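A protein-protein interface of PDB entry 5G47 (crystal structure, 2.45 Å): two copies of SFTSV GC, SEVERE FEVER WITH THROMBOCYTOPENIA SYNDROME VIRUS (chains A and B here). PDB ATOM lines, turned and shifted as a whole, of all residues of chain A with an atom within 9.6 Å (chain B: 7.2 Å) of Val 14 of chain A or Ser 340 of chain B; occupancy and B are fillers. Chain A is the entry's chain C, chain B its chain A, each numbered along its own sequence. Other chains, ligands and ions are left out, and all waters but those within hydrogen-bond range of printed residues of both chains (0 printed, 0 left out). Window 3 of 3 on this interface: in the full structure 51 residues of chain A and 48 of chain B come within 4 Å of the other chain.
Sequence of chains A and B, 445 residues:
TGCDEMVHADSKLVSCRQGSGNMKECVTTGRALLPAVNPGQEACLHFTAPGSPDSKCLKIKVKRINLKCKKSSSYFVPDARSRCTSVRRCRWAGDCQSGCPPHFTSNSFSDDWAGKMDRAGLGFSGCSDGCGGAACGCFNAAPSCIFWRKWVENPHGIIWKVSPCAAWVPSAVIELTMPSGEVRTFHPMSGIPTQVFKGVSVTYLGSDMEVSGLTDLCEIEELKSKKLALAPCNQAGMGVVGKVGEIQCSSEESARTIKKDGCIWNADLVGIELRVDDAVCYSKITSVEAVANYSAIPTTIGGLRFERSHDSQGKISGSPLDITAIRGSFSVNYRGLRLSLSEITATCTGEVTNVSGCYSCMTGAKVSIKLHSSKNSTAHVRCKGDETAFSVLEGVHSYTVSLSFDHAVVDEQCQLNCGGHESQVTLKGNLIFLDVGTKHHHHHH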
ATOM      1  N   SER A  11     -13.695   9.408 -21.052  1.00  0.00           N
ATOM      2  CA  SER A  11     -14.203  10.647 -20.484  1.00  0.00           C
ATOM      3  C   SER A  11     -14.218  11.742 -21.540  1.00  0.00           C
ATOM      4  O   SER A  11     -13.461  11.703 -22.512  1.00  0.00           O
ATOM      5  CB  SER A  11     -13.359  11.095 -19.282  1.00  0.00           C
ATOM      6  OG  SER A  11     -13.225  10.047 -18.336  1.00  0.00           O
ATOM      7  N   LYS A  12     -15.103  12.713 -21.335  1.00  0.00           N
ATOM      8  CA  LYS A  12     -15.144  13.942 -22.119  1.00  0.00           C
ATOM      9  C   LYS A  12     -14.680  15.081 -21.223  1.00  0.00           C
ATOM     10  O   LYS A  12     -15.279  15.329 -20.171  1.00  0.00           O
ATOM     11  CB  LYS A  12     -16.549  14.209 -22.658  1.00  0.00           C
ATOM     12  CG  LYS A  12     -17.079  13.120 -23.577  1.00  0.00           C
ATOM     13  CD  LYS A  12     -16.253  13.016 -24.850  1.00  0.00           C
ATOM     14  CE  LYS A  12     -16.786  11.921 -25.762  1.00  0.00           C
ATOM     15  NZ  LYS A  12     -16.070  11.887 -27.067  1.00  0.00           N
ATOM     16  N   LEU A  13     -13.617  15.766 -21.637  1.00  0.00           N
ATOM     17  CA  LEU A  13     -12.954  16.763 -20.811  1.00  0.00           C
ATOM     18  C   LEU A  13     -12.970  18.123 -21.494  1.00  0.00           C
ATOM     19  O   LEU A  13     -13.029  18.222 -22.722  1.00  0.00           O
ATOM     20  CB  LEU A  13     -11.505  16.355 -20.519  1.00  0.00           C
ATOM     21  CG  LEU A  13     -11.304  14.941 -19.971  1.00  0.00           C
ATOM     22  CD1 LEU A  13      -9.826  14.596 -19.894  1.00  0.00           C
ATOM     23  CD2 LEU A  13     -11.957  14.810 -18.609  1.00  0.00           C
ATOM     24  N   VAL A  14     -12.910  19.173 -20.678  1.00  0.00           N
ATOM     25  CA  VAL A  14     -12.798  20.548 -21.148  1.00  0.00           C
ATOM     26  C   VAL A  14     -11.405  21.035 -20.779  1.00  0.00           C
ATOM     27  O   VAL A  14     -11.128  21.327 -19.609  1.00  0.00           O
ATOM     28  CB  VAL A  14     -13.883  21.451 -20.543  1.00  0.00           C
ATOM     29  CG1 VAL A  14     -13.782  22.860 -21.115  1.00  0.00           C
ATOM     30  CG2 VAL A  14     -15.262  20.862 -20.794  1.00  0.00           C
ATOM     31  N   SER A  15     -10.519  21.105 -21.770  1.00  0.00           N
ATOM     32  CA  SER A  15      -9.146  21.545 -21.577  1.00  0.00           C
ATOM     33  C   SER A  15      -8.981  22.959 -22.117  1.00  0.00           C
ATOM     34  O   SER A  15      -9.500  23.289 -23.189  1.00  0.00           O
ATOM     35  CB  SER A  15      -8.160  20.601 -22.268  1.00  0.00           C
ATOM     36  OG  SER A  15      -8.417  20.529 -23.659  1.00  0.00           O
ATOM     37  N   CYS A  16      -8.255  23.789 -21.372  1.00  0.00           N
ATOM     38  CA  CYS A  16      -8.116  25.200 -21.690  1.00  0.00           C
ATOM     39  C   CYS A  16      -6.649  25.608 -21.645  1.00  0.00           C
ATOM     40  O   CYS A  16      -5.798  24.894 -21.109  1.00  0.00           O
ATOM     41  CB  CYS A  16      -8.931  26.069 -20.718  1.00  0.00           C
ATOM     42  SG  CYS A  16     -10.705  25.684 -20.626  1.00  0.00           S
ATOM     43  N   ARG A  17      -6.365  26.774 -22.220  1.00  0.00           N
ATOM     44  CA  ARG A  17      -5.018  27.340 -22.207  1.00  0.00           C
ATOM     45  C   ARG A  17      -5.006  28.695 -21.508  1.00  0.00           C
ATOM     46  O   ARG A  17      -4.604  29.703 -22.094  1.00  0.00           O
ATOM     47  CB  ARG A  17      -4.474  27.484 -23.629  1.00  0.00           C
ATOM     48  CG  ARG A  17      -4.177  26.169 -24.328  1.00  0.00           C
ATOM     49  CD  ARG A  17      -3.779  26.401 -25.777  1.00  0.00           C
ATOM     50  NE  ARG A  17      -3.584  25.148 -26.500  1.00  0.00           N
ATOM     51  CZ  ARG A  17      -3.514  25.055 -27.824  1.00  0.00           C
ATOM     52  NH1 ARG A  17      -3.627  26.143 -28.573  1.00  0.00           N
ATOM     53  NH2 ARG A  17      -3.335  23.874 -28.401  1.00  0.00           N
ATOM     54  N   LYS A  24      -7.911  32.787 -23.712  1.00  0.00           N
ATOM     55  CA  LYS A  24      -8.252  31.550 -23.018  1.00  0.00           C
ATOM     56  C   LYS A  24      -9.132  30.657 -23.887  1.00  0.00           C
ATOM     57  O   LYS A  24     -10.359  30.741 -23.835  1.00  0.00           O
ATOM     58  CB  LYS A  24      -8.959  31.852 -21.693  1.00  0.00           C
ATOM     59  CG  LYS A  24      -9.301  30.617 -20.866  1.00  0.00           C
ATOM     60  CD  LYS A  24     -10.253  30.956 -19.729  1.00  0.00           C
ATOM     61  CE  LYS A  24     -10.625  29.716 -18.933  1.00  0.00           C
ATOM     62  NZ  LYS A  24      -9.431  29.085 -18.309  1.00  0.00           N
ATOM     63  N   GLU A  25      -8.501  29.812 -24.697  1.00  0.00           N
ATOM     64  CA  GLU A  25      -9.251  28.835 -25.468  1.00  0.00           C
ATOM     65  C   GLU A  25      -9.721  27.707 -24.559  1.00  0.00           C
ATOM     66  O   GLU A  25      -9.139  27.447 -23.506  1.00  0.00           O
ATOM     67  CB  GLU A  25      -8.401  28.264 -26.604  1.00  0.00           C
ATOM     68  CG  GLU A  25      -7.231  27.406 -26.137  1.00  0.00           C
ATOM     69  CD  GLU A  25      -7.182  26.057 -26.833  1.00  0.00           C
ATOM     70  OE1 GLU A  25      -6.587  25.971 -27.927  1.00  0.00           O
ATOM     71  OE2 GLU A  25      -7.750  25.085 -26.290  1.00  0.00           O
ATOM     72  N   CYS A  26     -10.793  27.039 -24.977  1.00  0.00           N
ATOM     73  CA  CYS A  26     -11.302  25.870 -24.272  1.00  0.00           C
ATOM     74  C   CYS A  26     -11.966  24.953 -25.287  1.00  0.00           C
ATOM     75  O   CYS A  26     -12.788  25.407 -26.088  1.00  0.00           O
ATOM     76  CB  CYS A  26     -12.301  26.257 -23.175  1.00  0.00           C
ATOM     77  SG  CYS A  26     -11.612  27.125 -21.738  1.00  0.00           S
ATOM     78  N   VAL A  27     -11.605  23.672 -25.256  1.00  0.00           N
ATOM     79  CA  VAL A  27     -12.097  22.688 -26.212  1.00  0.00           C
ATOM     80  C   VAL A  27     -12.577  21.459 -25.454  1.00  0.00           C
ATOM     81  O   VAL A  27     -11.919  20.999 -24.513  1.00  0.00           O
ATOM     82  CB  VAL A  27     -11.011  22.297 -27.238  1.00  0.00           C
ATOM     83  CG1 VAL A  27     -11.555  21.290 -28.239  1.00  0.00           C
ATOM     84  CG2 VAL A  27     -10.476  23.528 -27.954  1.00  0.00           C
ATOM     85  N   THR A  28     -13.728  20.929 -25.863  1.00  0.00           N
ATOM     86  CA  THR A  28     -14.205  19.654 -25.349  1.00  0.00           C
ATOM     87  C   THR A  28     -13.474  18.521 -26.057  1.00  0.00           C
ATOM     88  O   THR A  28     -13.455  18.458 -27.290  1.00  0.00           O
ATOM     89  CB  THR A  28     -15.713  19.516 -25.549  1.00  0.00           C
ATOM     90  OG1 THR A  28     -16.390  20.554 -24.831  1.00  0.00           O
ATOM     91  CG2 THR A  28     -16.196  18.163 -25.048  1.00  0.00           C
ATOM     92  N   THR A  29     -12.874  17.627 -25.277  1.00  0.00           N
ATOM     93  CA  THR A  29     -12.045  16.563 -25.821  1.00  0.00           C
ATOM     94  C   THR A  29     -12.361  15.244 -25.132  1.00  0.00           C
ATOM     95  O   THR A  29     -12.818  15.215 -23.987  1.00  0.00           O
ATOM     96  CB  THR A  29     -10.550  16.884 -25.663  1.00  0.00           C
ATOM     97  OG1 THR A  29      -9.770  15.767 -26.108  1.00  0.00           O
ATOM     98  CG2 THR A  29     -10.218  17.180 -24.209  1.00  0.00           C
ATOM     99  N   GLY A  30     -12.108  14.154 -25.846  1.00  0.00           N
ATOM    100  CA  GLY A  30     -12.252  12.821 -25.301  1.00  0.00           C
ATOM    101  C   GLY A  30     -10.907  12.243 -24.902  1.00  0.00           C
ATOM    102  O   GLY A  30      -9.880  12.544 -25.506  1.00  0.00           O
ATOM    103  N   ARG A  31     -10.925  11.399 -23.872  1.00  0.00           N
ATOM    104  CA  ARG A  31      -9.696  10.821 -23.338  1.00  0.00           C
ATOM    105  C   ARG A  31     -10.006   9.447 -22.768  1.00  0.00           C
ATOM    106  O   ARG A  31     -10.829   9.324 -21.855  1.00  0.00           O
ATOM    107  CB  ARG A  31      -9.084  11.727 -22.267  1.00  0.00           C
ATOM    108  CG  ARG A  31      -7.703  11.297 -21.802  1.00  0.00           C
ATOM    109  CD  ARG A  31      -7.016  12.425 -21.054  1.00  0.00           C
ATOM    110  NE  ARG A  31      -6.935  13.635 -21.866  1.00  0.00           N
ATOM    111  CZ  ARG A  31      -6.604  14.832 -21.394  1.00  0.00           C
ATOM    112  NH1 ARG A  31      -6.326  14.984 -20.107  1.00  0.00           N
ATOM    113  NH2 ARG A  31      -6.558  15.878 -22.208  1.00  0.00           N
ATOM    114  N   ASN A 333      -5.900  10.487 -26.398  1.00  0.00           N
ATOM    115  CA  ASN A 333      -6.590  11.766 -26.483  1.00  0.00           C
ATOM    116  C   ASN A 333      -7.147  11.931 -27.891  1.00  0.00           C
ATOM    117  O   ASN A 333      -6.402  11.833 -28.873  1.00  0.00           O
ATOM    118  CB  ASN A 333      -5.645  12.921 -26.139  1.00  0.00           C
ATOM    119  CG  ASN A 333      -6.386  14.207 -25.833  1.00  0.00           C
ATOM    120  OD1 ASN A 333      -7.036  14.327 -24.795  1.00  0.00           O
ATOM    121  ND2 ASN A 333      -6.288  15.181 -26.732  1.00  0.00           N
ATOM    122  N   CYS B  44      -3.549  21.389 -13.215  1.00  0.00           N
ATOM    123  CA  CYS B  44      -4.280  22.601 -12.860  1.00  0.00           C
ATOM    124  C   CYS B  44      -5.758  22.352 -13.119  1.00  0.00           C
ATOM    125  O   CYS B  44      -6.170  22.181 -14.271  1.00  0.00           O
ATOM    126  CB  CYS B  44      -3.773  23.803 -13.657  1.00  0.00           C
ATOM    127  SG  CYS B  44      -1.992  24.081 -13.535  1.00  0.00           S
ATOM    128  N   LEU B  45      -6.548  22.328 -12.051  1.00  0.00           N
ATOM    129  CA  LEU B  45      -7.965  22.002 -12.118  1.00  0.00           C
ATOM    130  C   LEU B  45      -8.785  23.235 -11.771  1.00  0.00           C
ATOM    131  O   LEU B  45      -8.574  23.853 -10.720  1.00  0.00           O
ATOM    132  CB  LEU B  45      -8.312  20.850 -11.168  1.00  0.00           C
ATOM    133  CG  LEU B  45      -7.868  19.415 -11.492  1.00  0.00           C
ATOM    134  CD1 LEU B  45      -6.356  19.243 -11.417  1.00  0.00           C
ATOM    135  CD2 LEU B  45      -8.561  18.426 -10.563  1.00  0.00           C
ATOM    136  N   HIS B  46      -9.716  23.590 -12.652  1.00  0.00           N
ATOM    137  CA  HIS B  46     -10.612  24.720 -12.452  1.00  0.00           C
ATOM    138  C   HIS B  46     -12.006  24.207 -12.117  1.00  0.00           C
ATOM    139  O   HIS B  46     -12.512  23.296 -12.781  1.00  0.00           O
ATOM    140  CB  HIS B  46     -10.656  25.609 -13.696  1.00  0.00           C
ATOM    141  CG  HIS B  46      -9.378  26.345 -13.959  1.00  0.00           C
ATOM    142  ND1 HIS B  46      -9.040  27.506 -13.299  1.00  0.00           N
ATOM    143  CD2 HIS B  46      -8.359  26.086 -14.811  1.00  0.00           C
ATOM    144  CE1 HIS B  46      -7.867  27.930 -13.732  1.00  0.00           C
ATOM    145  NE2 HIS B  46      -7.432  27.087 -14.650  1.00  0.00           N
ATOM    146  N   PHE B  47     -12.620  24.792 -11.092  1.00  0.00           N
ATOM    147  CA  PHE B  47     -13.939  24.388 -10.616  1.00  0.00           C
ATOM    148  C   PHE B  47     -14.876  25.584 -10.664  1.00  0.00           C
ATOM    149  O   PHE B  47     -14.613  26.605 -10.021  1.00  0.00           O
ATOM    150  CB  PHE B  47     -13.864  23.836  -9.190  1.00  0.00           C
ATOM    151  CG  PHE B  47     -13.004  22.616  -9.056  1.00  0.00           C
ATOM    152  CD1 PHE B  47     -13.529  21.357  -9.294  1.00  0.00           C
ATOM    153  CD2 PHE B  47     -11.676  22.724  -8.688  1.00  0.00           C
ATOM    154  CE1 PHE B  47     -12.741  20.229  -9.170  1.00  0.00           C
ATOM    155  CE2 PHE B  47     -10.882  21.598  -8.563  1.00  0.00           C
ATOM    156  CZ  PHE B  47     -11.418  20.349  -8.805  1.00  0.00           C
ATOM    157  N   THR B  48     -15.971  25.451 -11.409  1.00  0.00           N
ATOM    158  CA  THR B  48     -16.991  26.486 -11.504  1.00  0.00           C
ATOM    159  C   THR B  48     -18.278  26.003 -10.848  1.00  0.00           C
ATOM    160  O   THR B  48     -18.633  24.826 -10.948  1.00  0.00           O
ATOM    161  CB  THR B  48     -17.280  26.863 -12.962  1.00  0.00           C
ATOM    162  OG1 THR B  48     -17.919  25.765 -13.626  1.00  0.00           O
ATOM    163  CG2 THR B  48     -15.996  27.207 -13.693  1.00  0.00           C
ATOM    164  N   SER B  55     -14.053  30.318 -12.217  1.00  0.00           N
ATOM    165  CA  SER B  55     -13.519  29.090 -11.647  1.00  0.00           C
ATOM    166  C   SER B  55     -12.582  29.359 -10.478  1.00  0.00           C
ATOM    167  O   SER B  55     -11.906  30.391 -10.419  1.00  0.00           O
ATOM    168  CB  SER B  55     -12.765  28.285 -12.709  1.00  0.00           C
ATOM    169  OG  SER B  55     -11.670  29.027 -13.218  1.00  0.00           O
ATOM    170  N   LYS B  56     -12.549  28.403  -9.550  1.00  0.00           N
ATOM    171  CA  LYS B  56     -11.504  28.323  -8.539  1.00  0.00           C
ATOM    172  C   LYS B  56     -10.421  27.374  -9.034  1.00  0.00           C
ATOM    173  O   LYS B  56     -10.723  26.285  -9.532  1.00  0.00           O
ATOM    174  CB  LYS B  56     -12.059  27.830  -7.200  1.00  0.00           C
ATOM    175  CG  LYS B  56     -13.000  28.793  -6.501  1.00  0.00           C
ATOM    176  CD  LYS B  56     -13.268  28.329  -5.076  1.00  0.00           C
ATOM    177  CE  LYS B  56     -14.193  29.282  -4.336  1.00  0.00           C
ATOM    178  NZ  LYS B  56     -15.559  29.311  -4.930  1.00  0.00           N
ATOM    179  N   TYR B 334     -15.014  16.126  -6.127  1.00  0.00           N
ATOM    180  CA  TYR B 334     -15.590  17.462  -6.109  1.00  0.00           C
ATOM    181  C   TYR B 334     -17.105  17.371  -6.195  1.00  0.00           C
ATOM    182  O   TYR B 334     -17.645  16.597  -6.993  1.00  0.00           O
ATOM    183  CB  TYR B 334     -15.036  18.327  -7.251  1.00  0.00           C
ATOM    184  CG  TYR B 334     -15.215  17.744  -8.637  1.00  0.00           C
ATOM    185  CD1 TYR B 334     -14.331  16.794  -9.134  1.00  0.00           C
ATOM    186  CD2 TYR B 334     -16.255  18.162  -9.459  1.00  0.00           C
ATOM    187  CE1 TYR B 334     -14.485  16.267 -10.400  1.00  0.00           C
ATOM    188  CE2 TYR B 334     -16.416  17.642 -10.729  1.00  0.00           C
ATOM    189  CZ  TYR B 334     -15.528  16.694 -11.194  1.00  0.00           C
ATOM    190  OH  TYR B 334     -15.684  16.172 -12.457  1.00  0.00           O
ATOM    191  N   ARG B 338     -18.214  22.067 -11.503  1.00  0.00           N
ATOM    192  CA  ARG B 338     -17.907  21.584 -12.842  1.00  0.00           C
ATOM    193  C   ARG B 338     -16.409  21.692 -13.078  1.00  0.00           C
ATOM    194  O   ARG B 338     -15.823  22.763 -12.885  1.00  0.00           O
ATOM    195  CB  ARG B 338     -18.671  22.376 -13.904  1.00  0.00           C
ATOM    196  CG  ARG B 338     -18.440  21.878 -15.321  1.00  0.00           C
ATOM    197  CD  ARG B 338     -19.207  22.697 -16.349  1.00  0.00           C
ATOM    198  NE  ARG B 338     -20.649  22.667 -16.120  1.00  0.00           N
ATOM    199  CZ  ARG B 338     -21.335  23.650 -15.546  1.00  0.00           C
ATOM    200  NH1 ARG B 338     -20.710  24.747 -15.143  1.00  0.00           N
ATOM    201  NH2 ARG B 338     -22.646  23.537 -15.378  1.00  0.00           N
ATOM    202  N   LEU B 339     -15.796  20.588 -13.496  1.00  0.00           N
ATOM    203  CA  LEU B 339     -14.352  20.518 -13.664  1.00  0.00           C
ATOM    204  C   LEU B 339     -13.948  20.941 -15.071  1.00  0.00           C
ATOM    205  O   LEU B 339     -14.552  20.511 -16.060  1.00  0.00           O
ATOM    206  CB  LEU B 339     -13.844  19.102 -13.384  1.00  0.00           C
ATOM    207  CG  LEU B 339     -12.378  18.825 -13.733  1.00  0.00           C
ATOM    208  CD1 LEU B 339     -11.442  19.685 -12.894  1.00  0.00           C
ATOM    209  CD2 LEU B 339     -12.041  17.348 -13.577  1.00  0.00           C
ATOM    210  N   SER B 340     -12.928  21.791 -15.150  1.00  0.00           N
ATOM    211  CA  SER B 340     -12.255  22.111 -16.398  1.00  0.00           C
ATOM    212  C   SER B 340     -10.755  22.087 -16.146  1.00  0.00           C
ATOM    213  O   SER B 340     -10.294  22.363 -15.034  1.00  0.00           O
ATOM    214  CB  SER B 340     -12.688  23.472 -16.957  1.00  0.00           C
ATOM    215  OG  SER B 340     -12.534  24.497 -15.992  1.00  0.00           O
ATOM    216  N   LEU B 341      -9.998  21.755 -17.185  1.00  0.00           N
ATOM    217  CA  LEU B 341      -8.569  21.516 -17.065  1.00  0.00           C
ATOM    218  C   LEU B 341      -7.783  22.579 -17.820  1.00  0.00           C
ATOM    219  O   LEU B 341      -8.201  23.033 -18.890  1.00  0.00           O
ATOM    220  CB  LEU B 341      -8.207  20.126 -17.600  1.00  0.00           C
ATOM    221  CG  LEU B 341      -9.026  18.965 -17.029  1.00  0.00           C
ATOM    222  CD1 LEU B 341      -8.689  17.662 -17.739  1.00  0.00           C
ATOM    223  CD2 LEU B 341      -8.801  18.838 -15.531  1.00  0.00           C
ATOM    224  N   SER B 342      -6.652  22.980 -17.248  1.00  0.00           N
ATOM    225  CA  SER B 342      -5.669  23.807 -17.933  1.00  0.00           C
ATOM    226  C   SER B 342      -4.566  22.885 -18.435  1.00  0.00           C
ATOM    227  O   SER B 342      -3.918  22.197 -17.639  1.00  0.00           O
ATOM    228  CB  SER B 342      -5.106  24.882 -17.001  1.00  0.00           C
ATOM    229  OG  SER B 342      -4.131  25.675 -17.658  1.00  0.00           O
ATOM    230  N   GLU B 343      -4.378  22.842 -19.752  1.00  0.00           N
ATOM    231  CA  GLU B 343      -3.422  21.927 -20.364  1.00  0.00           C
ATOM    232  C   GLU B 343      -2.747  22.624 -21.534  1.00  0.00           C
ATOM    233  O   GLU B 343      -3.423  23.088 -22.458  1.00  0.00           O
ATOM    234  CB  GLU B 343      -4.109  20.636 -20.825  1.00  0.00           C
ATOM    235  CG  GLU B 343      -4.612  19.758 -19.685  1.00  0.00           C
ATOM    236  CD  GLU B 343      -5.349  18.528 -20.171  1.00  0.00           C
ATOM    237  OE1 GLU B 343      -5.689  18.472 -21.372  1.00  0.00           O
ATOM    238  OE2 GLU B 343      -5.586  17.616 -19.350  1.00  0.00           O
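The backbone NH (N) of Leu 341 of chain B lies within hydrogen-bond range of the backbone carbonyl oxygen (O) of Val 14 of chain A (2.7 Å).
The backbone NH of Cys 16 of chain A lies within hydrogen-bond range of the backbone carbonyl oxygen of Leu 341 of chain B, at 2.6 Å.
N of Glu 343 of chain B is in hydrogen-bond range of O of Cys 16 of chain A (2.8 Å).
The side-chain carboxylate of Glu 343 of chain B is in salt-bridge range of the guanidinium group of Arg 31 of chain A.
N of Ser 342 of chain B sits at hydrogen-bond distance from O of Cys 44 of chain B (3.1 Å).
O of Ser 340 of chain B lies within hydrogen-bond range of N of His 46 of chain B (2.7 Å).
The backbone NH (N) of Leu 13 of chain A lies within hydrogen-bond range of the backbone carbonyl oxygen (O) of Thr 29 of chain A (2.5 Å).
O of Ser 15 of chain A sits at hydrogen-bond distance from N of Val 27 of chain A (3.0 Å).
The side-chain sulfur (SG) of Cys 26 of chain A forms a disulfide with the side-chain sulfur (SG) of Cys 16 of chain A.
NE of Arg 31 of chain A is in hydrogen-bond range of OD1 of Asn 333 of chain A.
Of chain B, only Ser 340 and Leu 341 come within 4 Å of Val 14 of chain A.
Of the printed residues of chain A, Ser 340 of chain B touches Val 14.
Leu 341 of chain B touches four residues of chain A.
Printed residues of chain A within 4 Å of Ser 342 of chain B: Cys 16 (3.4 Å).
Printed residues of chain B within 4 Å of Ser 15 of chain A: Leu 341 (3.2 Å) and Glu 343 (3.4 Å).
Of the printed residues of chain B, Leu 13 of chain A touches Leu 341.
Cys 26 of chain A touches none of the printed residues of chain B.
The nearest residue of chain B that does not touch Val 14 of chain A is Leu 339 of chain B (4.6 Å).
No position is printed for both chains.
Among the printed residues, merely in contact across the chains: Ser 15 of chain A with Leu 341 of chain B, Cys 16 of chain A with Ser 342 of chain B, Ser 15 of chain A with Glu 343 of chain B, Val 14 of chain A with Ser 340 of chain B, Arg 17 of chain A with Glu 343 of chain B and Leu 13 of chain A with Leu 341 of chain B.
Printed residues of chain B that touch a printed residue of chain A: Ser 340, Leu 341, Ser 342 and Glu 343.
Hydrophobic or aromatic side chains of chain B that line the printed part of chain A: Leu 341.
Along chain B the printed residues that touch a printed residue of chain A span positions 340 to 343.
Among the printed residues, Asp or Glu carboxylates within 4 Å of a Lys or Arg side-chain nitrogen of the other chain: Arg 31 of chain A with Glu 343 of chain B.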
